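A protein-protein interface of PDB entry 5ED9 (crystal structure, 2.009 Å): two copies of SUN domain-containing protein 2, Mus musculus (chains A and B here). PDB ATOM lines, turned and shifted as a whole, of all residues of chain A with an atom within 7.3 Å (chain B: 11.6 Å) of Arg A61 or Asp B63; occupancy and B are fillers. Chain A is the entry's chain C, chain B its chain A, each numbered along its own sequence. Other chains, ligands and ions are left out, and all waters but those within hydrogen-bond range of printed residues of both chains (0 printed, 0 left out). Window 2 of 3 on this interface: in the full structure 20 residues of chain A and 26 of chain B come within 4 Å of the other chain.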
ATOM      1  N   GLN A  55      18.225 -13.923   1.617  1.00  0.00           N
ATOM      2  CA  GLN A  55      17.898 -12.826   0.712  1.00  0.00           C
ATOM      3  C   GLN A  55      16.559 -12.173   1.056  1.00  0.00           C
ATOM      4  O   GLN A  55      16.415 -10.955   0.981  1.00  0.00           O
ATOM      5  CB  GLN A  55      17.894 -13.303  -0.737  1.00  0.00           C
ATOM      6  CG  GLN A  55      17.262 -12.313  -1.693  1.00  0.00           C
ATOM      7  CD  GLN A  55      17.620 -12.587  -3.135  1.00  0.00           C
ATOM      8  OE1 GLN A  55      17.526 -13.724  -3.610  1.00  0.00           O
ATOM      9  NE2 GLN A  55      18.047 -11.544  -3.844  1.00  0.00           N
ATOM     10  N   LYS A  56      15.583 -12.986   1.438  1.00  0.00           N
ATOM     11  CA  LYS A  56      14.285 -12.460   1.839  1.00  0.00           C
ATOM     12  C   LYS A  56      14.352 -11.630   3.127  1.00  0.00           C
ATOM     13  O   LYS A  56      13.659 -10.617   3.259  1.00  0.00           O
ATOM     14  CB  LYS A  56      13.271 -13.594   1.973  1.00  0.00           C
ATOM     15  CG  LYS A  56      13.023 -14.320   0.655  1.00  0.00           C
ATOM     16  CD  LYS A  56      11.739 -15.127   0.701  1.00  0.00           C
ATOM     17  CE  LYS A  56      11.291 -15.515  -0.697  1.00  0.00           C
ATOM     18  NZ  LYS A  56       9.983 -16.227  -0.664  1.00  0.00           N
ATOM     19  N   ILE A  57      15.185 -12.055   4.071  1.00  0.00           N
ATOM     20  CA  ILE A  57      15.394 -11.294   5.299  1.00  0.00           C
ATOM     21  C   ILE A  57      15.957  -9.909   4.993  1.00  0.00           C
ATOM     22  O   ILE A  57      15.480  -8.901   5.529  1.00  0.00           O
ATOM     23  CB  ILE A  57      16.342 -12.021   6.270  1.00  0.00           C
ATOM     24  CG1 ILE A  57      15.676 -13.284   6.814  1.00  0.00           C
ATOM     25  CG2 ILE A  57      16.738 -11.109   7.418  1.00  0.00           C
ATOM     26  CD1 ILE A  57      16.556 -14.066   7.749  1.00  0.00           C
ATOM     27  N   GLN A  58      16.959  -9.857   4.122  1.00  0.00           N
ATOM     28  CA  GLN A  58      17.557  -8.586   3.726  1.00  0.00           C
ATOM     29  C   GLN A  58      16.542  -7.698   3.011  1.00  0.00           C
ATOM     30  O   GLN A  58      16.550  -6.475   3.180  1.00  0.00           O
ATOM     31  CB  GLN A  58      18.790  -8.815   2.851  1.00  0.00           C
ATOM     32  CG  GLN A  58      19.814  -9.755   3.471  1.00  0.00           C
ATOM     33  CD  GLN A  58      20.156  -9.381   4.900  1.00  0.00           C
ATOM     34  OE1 GLN A  58      19.948 -10.165   5.832  1.00  0.00           O
ATOM     35  NE2 GLN A  58      20.695  -8.181   5.080  1.00  0.00           N
ATOM     36  N   ALA A  59      15.663  -8.318   2.225  1.00  0.00           N
ATOM     37  CA  ALA A  59      14.594  -7.587   1.553  1.00  0.00           C
ATOM     38  C   ALA A  59      13.647  -6.950   2.571  1.00  0.00           C
ATOM     39  O   ALA A  59      13.176  -5.827   2.384  1.00  0.00           O
ATOM     40  CB  ALA A  59      13.827  -8.509   0.623  1.00  0.00           C
ATOM     41  N   ALA A  60      13.365  -7.679   3.645  1.00  0.00           N
ATOM     42  CA  ALA A  60      12.478  -7.184   4.689  1.00  0.00           C
ATOM     43  C   ALA A  60      13.081  -5.984   5.413  1.00  0.00           C
ATOM     44  O   ALA A  60      12.372  -5.036   5.751  1.00  0.00           O
ATOM     45  CB  ALA A  60      12.145  -8.292   5.675  1.00  0.00           C
ATOM     46  N   ARG A  61      14.390  -6.013   5.642  1.00  0.00           N
ATOM     47  CA  ARG A  61      15.031  -4.912   6.349  1.00  0.00           C
ATOM     48  C   ARG A  61      15.288  -3.705   5.443  1.00  0.00           C
ATOM     49  O   ARG A  61      15.367  -2.573   5.919  1.00  0.00           O
ATOM     50  CB  ARG A  61      16.307  -5.364   7.069  1.00  0.00           C
ATOM     51  CG  ARG A  61      17.566  -5.377   6.226  1.00  0.00           C
ATOM     52  CD  ARG A  61      18.782  -5.419   7.138  1.00  0.00           C
ATOM     53  NE  ARG A  61      20.045  -5.502   6.411  1.00  0.00           N
ATOM     54  CZ  ARG A  61      21.239  -5.481   6.996  1.00  0.00           C
ATOM     55  NH1 ARG A  61      21.327  -5.374   8.316  1.00  0.00           N
ATOM     56  NH2 ARG A  61      22.344  -5.565   6.264  1.00  0.00           N
ATOM     57  N   ALA A  62      15.410  -3.944   4.142  1.00  0.00           N
ATOM     58  CA  ALA A  62      15.511  -2.846   3.189  1.00  0.00           C
ATOM     59  C   ALA A  62      14.148  -2.171   3.014  1.00  0.00           C
ATOM     60  O   ALA A  62      14.061  -0.950   2.851  1.00  0.00           O
ATOM     61  CB  ALA A  62      16.039  -3.343   1.855  1.00  0.00           C
ATOM     62  N   ASP A  63      13.086  -2.975   3.052  1.00  0.00           N
ATOM     63  CA  ASP A  63      11.727  -2.464   2.926  1.00  0.00           C
ATOM     64  C   ASP A  63      11.355  -1.562   4.098  1.00  0.00           C
ATOM     65  O   ASP A  63      10.760  -0.501   3.903  1.00  0.00           O
ATOM     66  CB  ASP A  63      10.723  -3.613   2.805  1.00  0.00           C
ATOM     67  CG  ASP A  63       9.283  -3.130   2.817  1.00  0.00           C
ATOM     68  OD1 ASP A  63       8.773  -2.741   1.744  1.00  0.00           O
ATOM     69  OD2 ASP A  63       8.663  -3.137   3.900  1.00  0.00           O
ATOM     70  N   VAL A  64      11.698  -1.993   5.309  1.00  0.00           N
ATOM     71  CA  VAL A  64      11.515  -1.161   6.495  1.00  0.00           C
ATOM     72  C   VAL A  64      12.130   0.217   6.271  1.00  0.00           C
ATOM     73  O   VAL A  64      11.449   1.232   6.379  1.00  0.00           O
ATOM     74  CB  VAL A  64      12.137  -1.806   7.756  1.00  0.00           C
ATOM     75  CG1 VAL A  64      12.461  -0.750   8.809  1.00  0.00           C
ATOM     76  CG2 VAL A  64      11.207  -2.847   8.329  1.00  0.00           C
ATOM     77  N   GLU A  65      13.411   0.239   5.918  1.00  0.00           N
ATOM     78  CA  GLU A  65      14.138   1.488   5.712  1.00  0.00           C
ATOM     79  C   GLU A  65      13.518   2.357   4.612  1.00  0.00           C
ATOM     80  O   GLU A  65      13.530   3.585   4.700  1.00  0.00           O
ATOM     81  CB  GLU A  65      15.608   1.194   5.404  1.00  0.00           C
ATOM     82  CG  GLU A  65      16.488   2.425   5.285  1.00  0.00           C
ATOM     83  CD  GLU A  65      17.942   2.075   5.026  1.00  0.00           C
ATOM     84  OE1 GLU A  65      18.665   2.927   4.466  1.00  0.00           O
ATOM     85  OE2 GLU A  65      18.359   0.952   5.381  1.00  0.00           O
ATOM     86  N   SER A  66      12.967   1.717   3.585  1.00  0.00           N
ATOM     87  CA  SER A  66      12.341   2.437   2.481  1.00  0.00           C
ATOM     88  C   SER A  66      10.959   2.958   2.843  1.00  0.00           C
ATOM     89  O   SER A  66      10.604   4.082   2.494  1.00  0.00           O
ATOM     90  CB  SER A  66      12.231   1.537   1.247  1.00  0.00           C
ATOM     91  OG  SER A  66      13.510   1.144   0.778  1.00  0.00           O
ATOM     92  N   PRO B  54      16.310 -18.206  12.868  1.00  0.00           N
ATOM     93  CA  PRO B  54      15.848 -17.296  13.928  1.00  0.00           C
ATOM     94  C   PRO B  54      16.932 -16.331  14.412  1.00  0.00           C
ATOM     95  O   PRO B  54      16.639 -15.180  14.738  1.00  0.00           O
ATOM     96  CB  PRO B  54      15.463 -18.250  15.058  1.00  0.00           C
ATOM     97  CG  PRO B  54      15.085 -19.508  14.362  1.00  0.00           C
ATOM     98  CD  PRO B  54      16.034 -19.614  13.209  1.00  0.00           C
ATOM     99  N   GLN B  55      18.170 -16.804  14.454  1.00  0.00           N
ATOM    100  CA  GLN B  55      19.309 -15.975  14.830  1.00  0.00           C
ATOM    101  C   GLN B  55      19.540 -14.868  13.801  1.00  0.00           C
ATOM    102  O   GLN B  55      19.985 -13.766  14.135  1.00  0.00           O
ATOM    103  CB  GLN B  55      20.556 -16.852  14.971  1.00  0.00           C
ATOM    104  CG  GLN B  55      21.870 -16.104  15.081  1.00  0.00           C
ATOM    105  CD  GLN B  55      23.061 -17.048  15.157  1.00  0.00           C
ATOM    106  OE1 GLN B  55      22.914 -18.227  15.492  1.00  0.00           O
ATOM    107  NE2 GLN B  55      24.247 -16.535  14.842  1.00  0.00           N
ATOM    108  N   LYS B  56      19.222 -15.168  12.547  1.00  0.00           N
ATOM    109  CA  LYS B  56      19.425 -14.220  11.460  1.00  0.00           C
ATOM    110  C   LYS B  56      18.365 -13.121  11.475  1.00  0.00           C
ATOM    111  O   LYS B  56      18.645 -11.968  11.138  1.00  0.00           O
ATOM    112  CB  LYS B  56      19.403 -14.958  10.123  1.00  0.00           C
ATOM    113  CG  LYS B  56      20.479 -14.517   9.153  1.00  0.00           C
ATOM    114  CD  LYS B  56      20.895 -15.667   8.251  1.00  0.00           C
ATOM    115  CE  LYS B  56      21.488 -16.807   9.063  1.00  0.00           C
ATOM    116  NZ  LYS B  56      22.064 -17.869   8.189  1.00  0.00           N
ATOM    117  N   ILE B  57      17.148 -13.484  11.864  1.00  0.00           N
ATOM    118  CA  ILE B  57      16.044 -12.531  11.923  1.00  0.00           C
ATOM    119  C   ILE B  57      16.242 -11.508  13.042  1.00  0.00           C
ATOM    120  O   ILE B  57      15.941 -10.326  12.874  1.00  0.00           O
ATOM    121  CB  ILE B  57      14.694 -13.251  12.103  1.00  0.00           C
ATOM    122  CG1 ILE B  57      14.351 -14.043  10.840  1.00  0.00           C
ATOM    123  CG2 ILE B  57      13.592 -12.262  12.422  1.00  0.00           C
ATOM    124  CD1 ILE B  57      12.951 -14.614  10.832  1.00  0.00           C
ATOM    125  N   GLN B  58      16.769 -11.965  14.174  1.00  0.00           N
ATOM    126  CA  GLN B  58      16.984 -11.090  15.323  1.00  0.00           C
ATOM    127  C   GLN B  58      18.127 -10.107  15.095  1.00  0.00           C
ATOM    128  O   GLN B  58      18.098  -8.986  15.602  1.00  0.00           O
ATOM    129  CB  GLN B  58      17.235 -11.905  16.593  1.00  0.00           C
ATOM    130  CG  GLN B  58      16.159 -12.935  16.887  1.00  0.00           C
ATOM    131  CD  GLN B  58      14.762 -12.400  16.647  1.00  0.00           C
ATOM    132  OE1 GLN B  58      14.377 -11.365  17.192  1.00  0.00           O
ATOM    133  NE2 GLN B  58      13.995 -13.102  15.818  1.00  0.00           N
ATOM    134  N   ALA B  59      19.133 -10.534  14.341  1.00  0.00           N
ATOM    135  CA  ALA B  59      20.249  -9.662  14.000  1.00  0.00           C
ATOM    136  C   ALA B  59      19.757  -8.482  13.175  1.00  0.00           C
ATOM    137  O   ALA B  59      20.060  -7.331  13.482  1.00  0.00           O
ATOM    138  CB  ALA B  59      21.310 -10.429  13.240  1.00  0.00           C
ATOM    139  N   ALA B  60      18.994  -8.778  12.127  1.00  0.00           N
ATOM    140  CA  ALA B  60      18.412  -7.745  11.281  1.00  0.00           C
ATOM    141  C   ALA B  60      17.425  -6.897  12.076  1.00  0.00           C
ATOM    142  O   ALA B  60      17.433  -5.671  11.977  1.00  0.00           O
ATOM    143  CB  ALA B  60      17.731  -8.372  10.077  1.00  0.00           C
ATOM    144  N   ARG B  61      16.583  -7.561  12.863  1.00  0.00           N
ATOM    145  CA  ARG B  61      15.620  -6.888  13.729  1.00  0.00           C
ATOM    146  C   ARG B  61      16.306  -5.875  14.639  1.00  0.00           C
ATOM    147  O   ARG B  61      15.850  -4.742  14.776  1.00  0.00           O
ATOM    148  CB  ARG B  61      14.874  -7.915  14.580  1.00  0.00           C
ATOM    149  CG  ARG B  61      13.786  -7.339  15.468  1.00  0.00           C
ATOM    150  CD  ARG B  61      13.460  -8.309  16.590  1.00  0.00           C
ATOM    151  NE  ARG B  61      12.029  -8.389  16.869  1.00  0.00           N
ATOM    152  CZ  ARG B  61      11.494  -9.193  17.784  1.00  0.00           C
ATOM    153  NH1 ARG B  61      10.180  -9.206  17.975  1.00  0.00           N
ATOM    154  NH2 ARG B  61      12.271  -9.984  18.510  1.00  0.00           N
ATOM    155  N   ALA B  62      17.408  -6.289  15.255  1.00  0.00           N
ATOM    156  CA  ALA B  62      18.173  -5.404  16.124  1.00  0.00           C
ATOM    157  C   ALA B  62      18.968  -4.390  15.311  1.00  0.00           C
ATOM    158  O   ALA B  62      19.204  -3.270  15.762  1.00  0.00           O
ATOM    159  CB  ALA B  62      19.102  -6.210  17.023  1.00  0.00           C
ATOM    160  N   ASP B  63      19.380  -4.790  14.112  1.00  0.00           N
ATOM    161  CA  ASP B  63      20.142  -3.912  13.231  1.00  0.00           C
ATOM    162  C   ASP B  63      19.323  -2.701  12.797  1.00  0.00           C
ATOM    163  O   ASP B  63      19.843  -1.586  12.715  1.00  0.00           O
ATOM    164  CB  ASP B  63      20.623  -4.675  11.995  1.00  0.00           C
ATOM    165  CG  ASP B  63      21.426  -3.805  11.052  1.00  0.00           C
ATOM    166  OD1 ASP B  63      22.671  -3.816  11.150  1.00  0.00           O
ATOM    167  OD2 ASP B  63      20.813  -3.107  10.215  1.00  0.00           O
ATOM    168  N   VAL B  64      18.044  -2.928  12.514  1.00  0.00           N
ATOM    169  CA  VAL B  64      17.151  -1.856  12.083  1.00  0.00           C
ATOM    170  C   VAL B  64      17.014  -0.761  13.139  1.00  0.00           C
ATOM    171  O   VAL B  64      17.172   0.424  12.841  1.00  0.00           O
ATOM    172  CB  VAL B  64      15.750  -2.401  11.711  1.00  0.00           C
ATOM    173  CG1 VAL B  64      14.713  -1.285  11.732  1.00  0.00           C
ATOM    174  CG2 VAL B  64      15.783  -3.086  10.349  1.00  0.00           C
ATOM    175  N   GLU B  65      16.741  -1.165  14.376  1.00  0.00           N
ATOM    176  CA  GLU B  65      16.446  -0.228  15.455  1.00  0.00           C
ATOM    177  C   GLU B  65      17.682   0.503  15.979  1.00  0.00           C
ATOM    178  O   GLU B  65      17.583   1.317  16.898  1.00  0.00           O
ATOM    179  CB  GLU B  65      15.724  -0.950  16.593  1.00  0.00           C
ATOM    180  CG  GLU B  65      14.448  -1.646  16.148  1.00  0.00           C
ATOM    181  CD  GLU B  65      14.113  -2.863  16.996  1.00  0.00           C
ATOM    182  OE1 GLU B  65      14.498  -2.885  18.187  1.00  0.00           O
ATOM    183  OE2 GLU B  65      13.472  -3.801  16.468  1.00  0.00           O
ATOM    184  N   SER B  66      18.840   0.204  15.397  1.00  0.00           N
ATOM    185  CA  SER B  66      20.065   0.920  15.731  1.00  0.00           C
ATOM    186  C   SER B  66      20.340   1.981  14.674  1.00  0.00           C
ATOM    187  O   SER B  66      21.053   2.952  14.931  1.00  0.00           O
ATOM    188  CB  SER B  66      21.249  -0.040  15.838  1.00  0.00           C
ATOM    189  OG  SER B  66      21.680  -0.455  14.555  1.00  0.00           O
ATOM    190  N   GLN B  67      19.776   1.778  13.485  1.00  0.00           N
ATOM    191  CA  GLN B  67      19.898   2.738  12.392  1.00  0.00           C
ATOM    192  C   GLN B  67      18.762   3.750  12.429  1.00  0.00           C
ATOM    193  O   GLN B  67      18.706   4.659  11.604  1.00  0.00           O
ATOM    194  CB  GLN B  67      19.888   2.019  11.040  1.00  0.00           C
ATOM    195  CG  GLN B  67      21.067   1.103  10.775  1.00  0.00           C
ATOM    196  CD  GLN B  67      20.969   0.433   9.410  1.00  0.00           C
ATOM    197  OE1 GLN B  67      20.824   1.102   8.380  1.00  0.00           O
ATOM    198  NE2 GLN B  67      21.040  -0.895   9.399  1.00  0.00           N
ATOM    199  N   PHE B  68      17.858   3.582  13.385  1.00  0.00           N
ATOM    200  CA  PHE B  68      16.639   4.385  13.432  1.00  0.00           C
ATOM    201  C   PHE B  68      16.805   5.904  13.669  1.00  0.00           C
ATOM    202  O   PHE B  68      16.221   6.698  12.928  1.00  0.00           O
ATOM    203  CB  PHE B  68      15.642   3.791  14.429  1.00  0.00           C
ATOM    204  CG  PHE B  68      14.215   3.878  13.977  1.00  0.00           C
ATOM    205  CD1 PHE B  68      13.588   5.104  13.828  1.00  0.00           C
ATOM    206  CD2 PHE B  68      13.499   2.731  13.706  1.00  0.00           C
ATOM    207  CE1 PHE B  68      12.277   5.183  13.416  1.00  0.00           C
ATOM    208  CE2 PHE B  68      12.204   2.808  13.291  1.00  0.00           C
ATOM    209  CZ  PHE B  68      11.584   4.033  13.147  1.00  0.00           C
ATOM    210  N   PRO B  69      17.553   6.318  14.718  1.00  0.00           N
ATOM    211  CA  PRO B  69      17.692   7.766  14.933  1.00  0.00           C
ATOM    212  C   PRO B  69      18.386   8.414  13.750  1.00  0.00           C
ATOM    213  O   PRO B  69      18.087   9.554  13.390  1.00  0.00           O
ATOM    214  CB  PRO B  69      18.598   7.860  16.167  1.00  0.00           C
ATOM    215  CG  PRO B  69      18.497   6.541  16.830  1.00  0.00           C
ATOM    216  CD  PRO B  69      18.311   5.551  15.722  1.00  0.00           C
ATOM    217  N   ASP B  70      19.302   7.666  13.146  1.00  0.00           N
ATOM    218  CA  ASP B  70      20.033   8.129  11.980  1.00  0.00           C
ATOM    219  C   ASP B  70      19.102   8.269  10.779  1.00  0.00           C
ATOM    220  O   ASP B  70      19.357   9.066   9.879  1.00  0.00           O
ATOM    221  CB  ASP B  70      21.176   7.165  11.663  1.00  0.00           C
ATOM    222  CG  ASP B  70      22.197   7.761  10.722  1.00  0.00           C
ATOM    223  OD1 ASP B  70      22.267   9.007  10.634  1.00  0.00           O
ATOM    224  OD2 ASP B  70      22.935   6.987  10.076  1.00  0.00           O
ATOM    225  N   TRP B  71      18.017   7.498  10.775  1.00  0.00           N
ATOM    226  CA  TRP B  71      17.044   7.556   9.686  1.00  0.00           C
ATOM    227  C   TRP B  71      16.197   8.823   9.749  1.00  0.00           C
ATOM    228  O   TRP B  71      15.804   9.365   8.716  1.00  0.00           O
ATOM    229  CB  TRP B  71      16.157   6.305   9.671  1.00  0.00           C
ATOM    230  CG  TRP B  71      16.864   5.084   9.165  1.00  0.00           C
ATOM    231  CD1 TRP B  71      18.070   5.044   8.519  1.00  0.00           C
ATOM    232  CD2 TRP B  71      16.429   3.719   9.260  1.00  0.00           C
ATOM    233  NE1 TRP B  71      18.403   3.749   8.206  1.00  0.00           N
ATOM    234  CE2 TRP B  71      17.403   2.914   8.657  1.00  0.00           C
ATOM    235  CE3 TRP B  71      15.288   3.107   9.807  1.00  0.00           C
ATOM    236  CZ2 TRP B  71      17.296   1.525   8.575  1.00  0.00           C
ATOM    237  CZ3 TRP B  71      15.178   1.725   9.725  1.00  0.00           C
ATOM    238  CH2 TRP B  71      16.174   0.952   9.115  1.00  0.00           C
ATOM    239  N   GLN B  74      18.664  11.545   8.482  1.00  0.00           N
ATOM    240  CA  GLN B  74      18.758  11.497   7.025  1.00  0.00           C
ATOM    241  C   GLN B  74      17.534  12.127   6.380  1.00  0.00           C
ATOM    242  O   GLN B  74      17.627  12.770   5.335  1.00  0.00           O
ATOM    243  CB  GLN B  74      18.878  10.051   6.542  1.00  0.00           C
ATOM    244  CG  GLN B  74      20.248   9.428   6.712  1.00  0.00           C
ATOM    245  CD  GLN B  74      20.274   7.968   6.292  1.00  0.00           C
ATOM    246  OE1 GLN B  74      19.249   7.284   6.319  1.00  0.00           O
ATOM    247  NE2 GLN B  74      21.447   7.486   5.898  1.00  0.00           N
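Ile A57 touches Lys B56, but with the chains exchanged Lys A56 does not touch Ile B57 (8.1 Å).
Ile B57 touches its own counterpart, Ile A57.
Ile A57 touches Ala B60, but with the chains exchanged Ala A60 does not touch Ile B57 (8.0 Å).
Val B64 touches its own counterpart, Val A64.
Positions printed for both chains: 55, 56, 57, 58, 59, 60, 61, 62, 63, 64, 65 and 66.
Of the 8 pairs that touch across the chains among the printed residues, 2 have their exchanged pair printed and touching as well.
Among the printed residues, pairs that only touch across the chains: Ile A57 with Lys B56 (3.8 Å), Ile A57 with Ile B57 (3.8 Å), Ile A57 with Ala B60 (3.9 Å), Val A64 with Val B64 (3.7 Å), Val A64 with Trp B71 (3.8 Å), Glu A65 with Gln B67 (3.9 Å) and Glu A65 with Trp B71 (3.4 Å).
Printed residues of chain B that touch a printed residue of chain A: Lys B56, Ile B57, Ala B60, Asp B63, Val B64, Gln B67 and Trp B71.
Of the 12 printed residues of chain A, 4 touch a printed residue of chain B.
Printed residues of chain A that touch a printed residue of chain B: Ile A57, Arg A61, Val A64 and Glu A65.
Hydrophobic or aromatic side chains of chain A within 4 Å of the printed part of chain B: Ile A57 and Val A64.
Among the printed residues, Asp or Glu carboxylates within 4 Å of a Lys or Arg side-chain nitrogen of the other chain: Arg A61 with Asp B63 (3.0 Å).
The guanidinium group (NE) of Arg A61 sits close to the side-chain amide nitrogen (NE2) of Gln A58 (3.1 Å).
O of Asp B63 lies within hydrogen-bond range of OG of Ser B66 (2.8 Å).
Of chain B, only Asp B63 (3.0 Å) comes within 4 Å of Arg A61.
Asp B63 touches one residue of chain A.
No residue of chain B comes within 4 Å of Gln A58.
No residue of chain B comes within 4 Å of Ala A59.
No residue of chain B comes within 4 Å of Ala A60.
Val A64 touches two residues of chain B.
Of chain B, only Gln B67 and Trp B71 come within 4 Å of Glu A65.
Of the printed residues of chain A, Ala B60 touches Ile A57.
Printed residues of chain A within 4 Å of Val B64: Val A64.
Glu B65 touches none of the printed residues of chain A.
Ala B59 touches none of the printed residues of chain A.
The nearest printed residue of chain A that does not touch Ile B57 is Gln A58 (7.4 Å).
The guanidinium group of Arg A61 is in salt-bridge range of the side-chain carboxylate of Asp B63.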
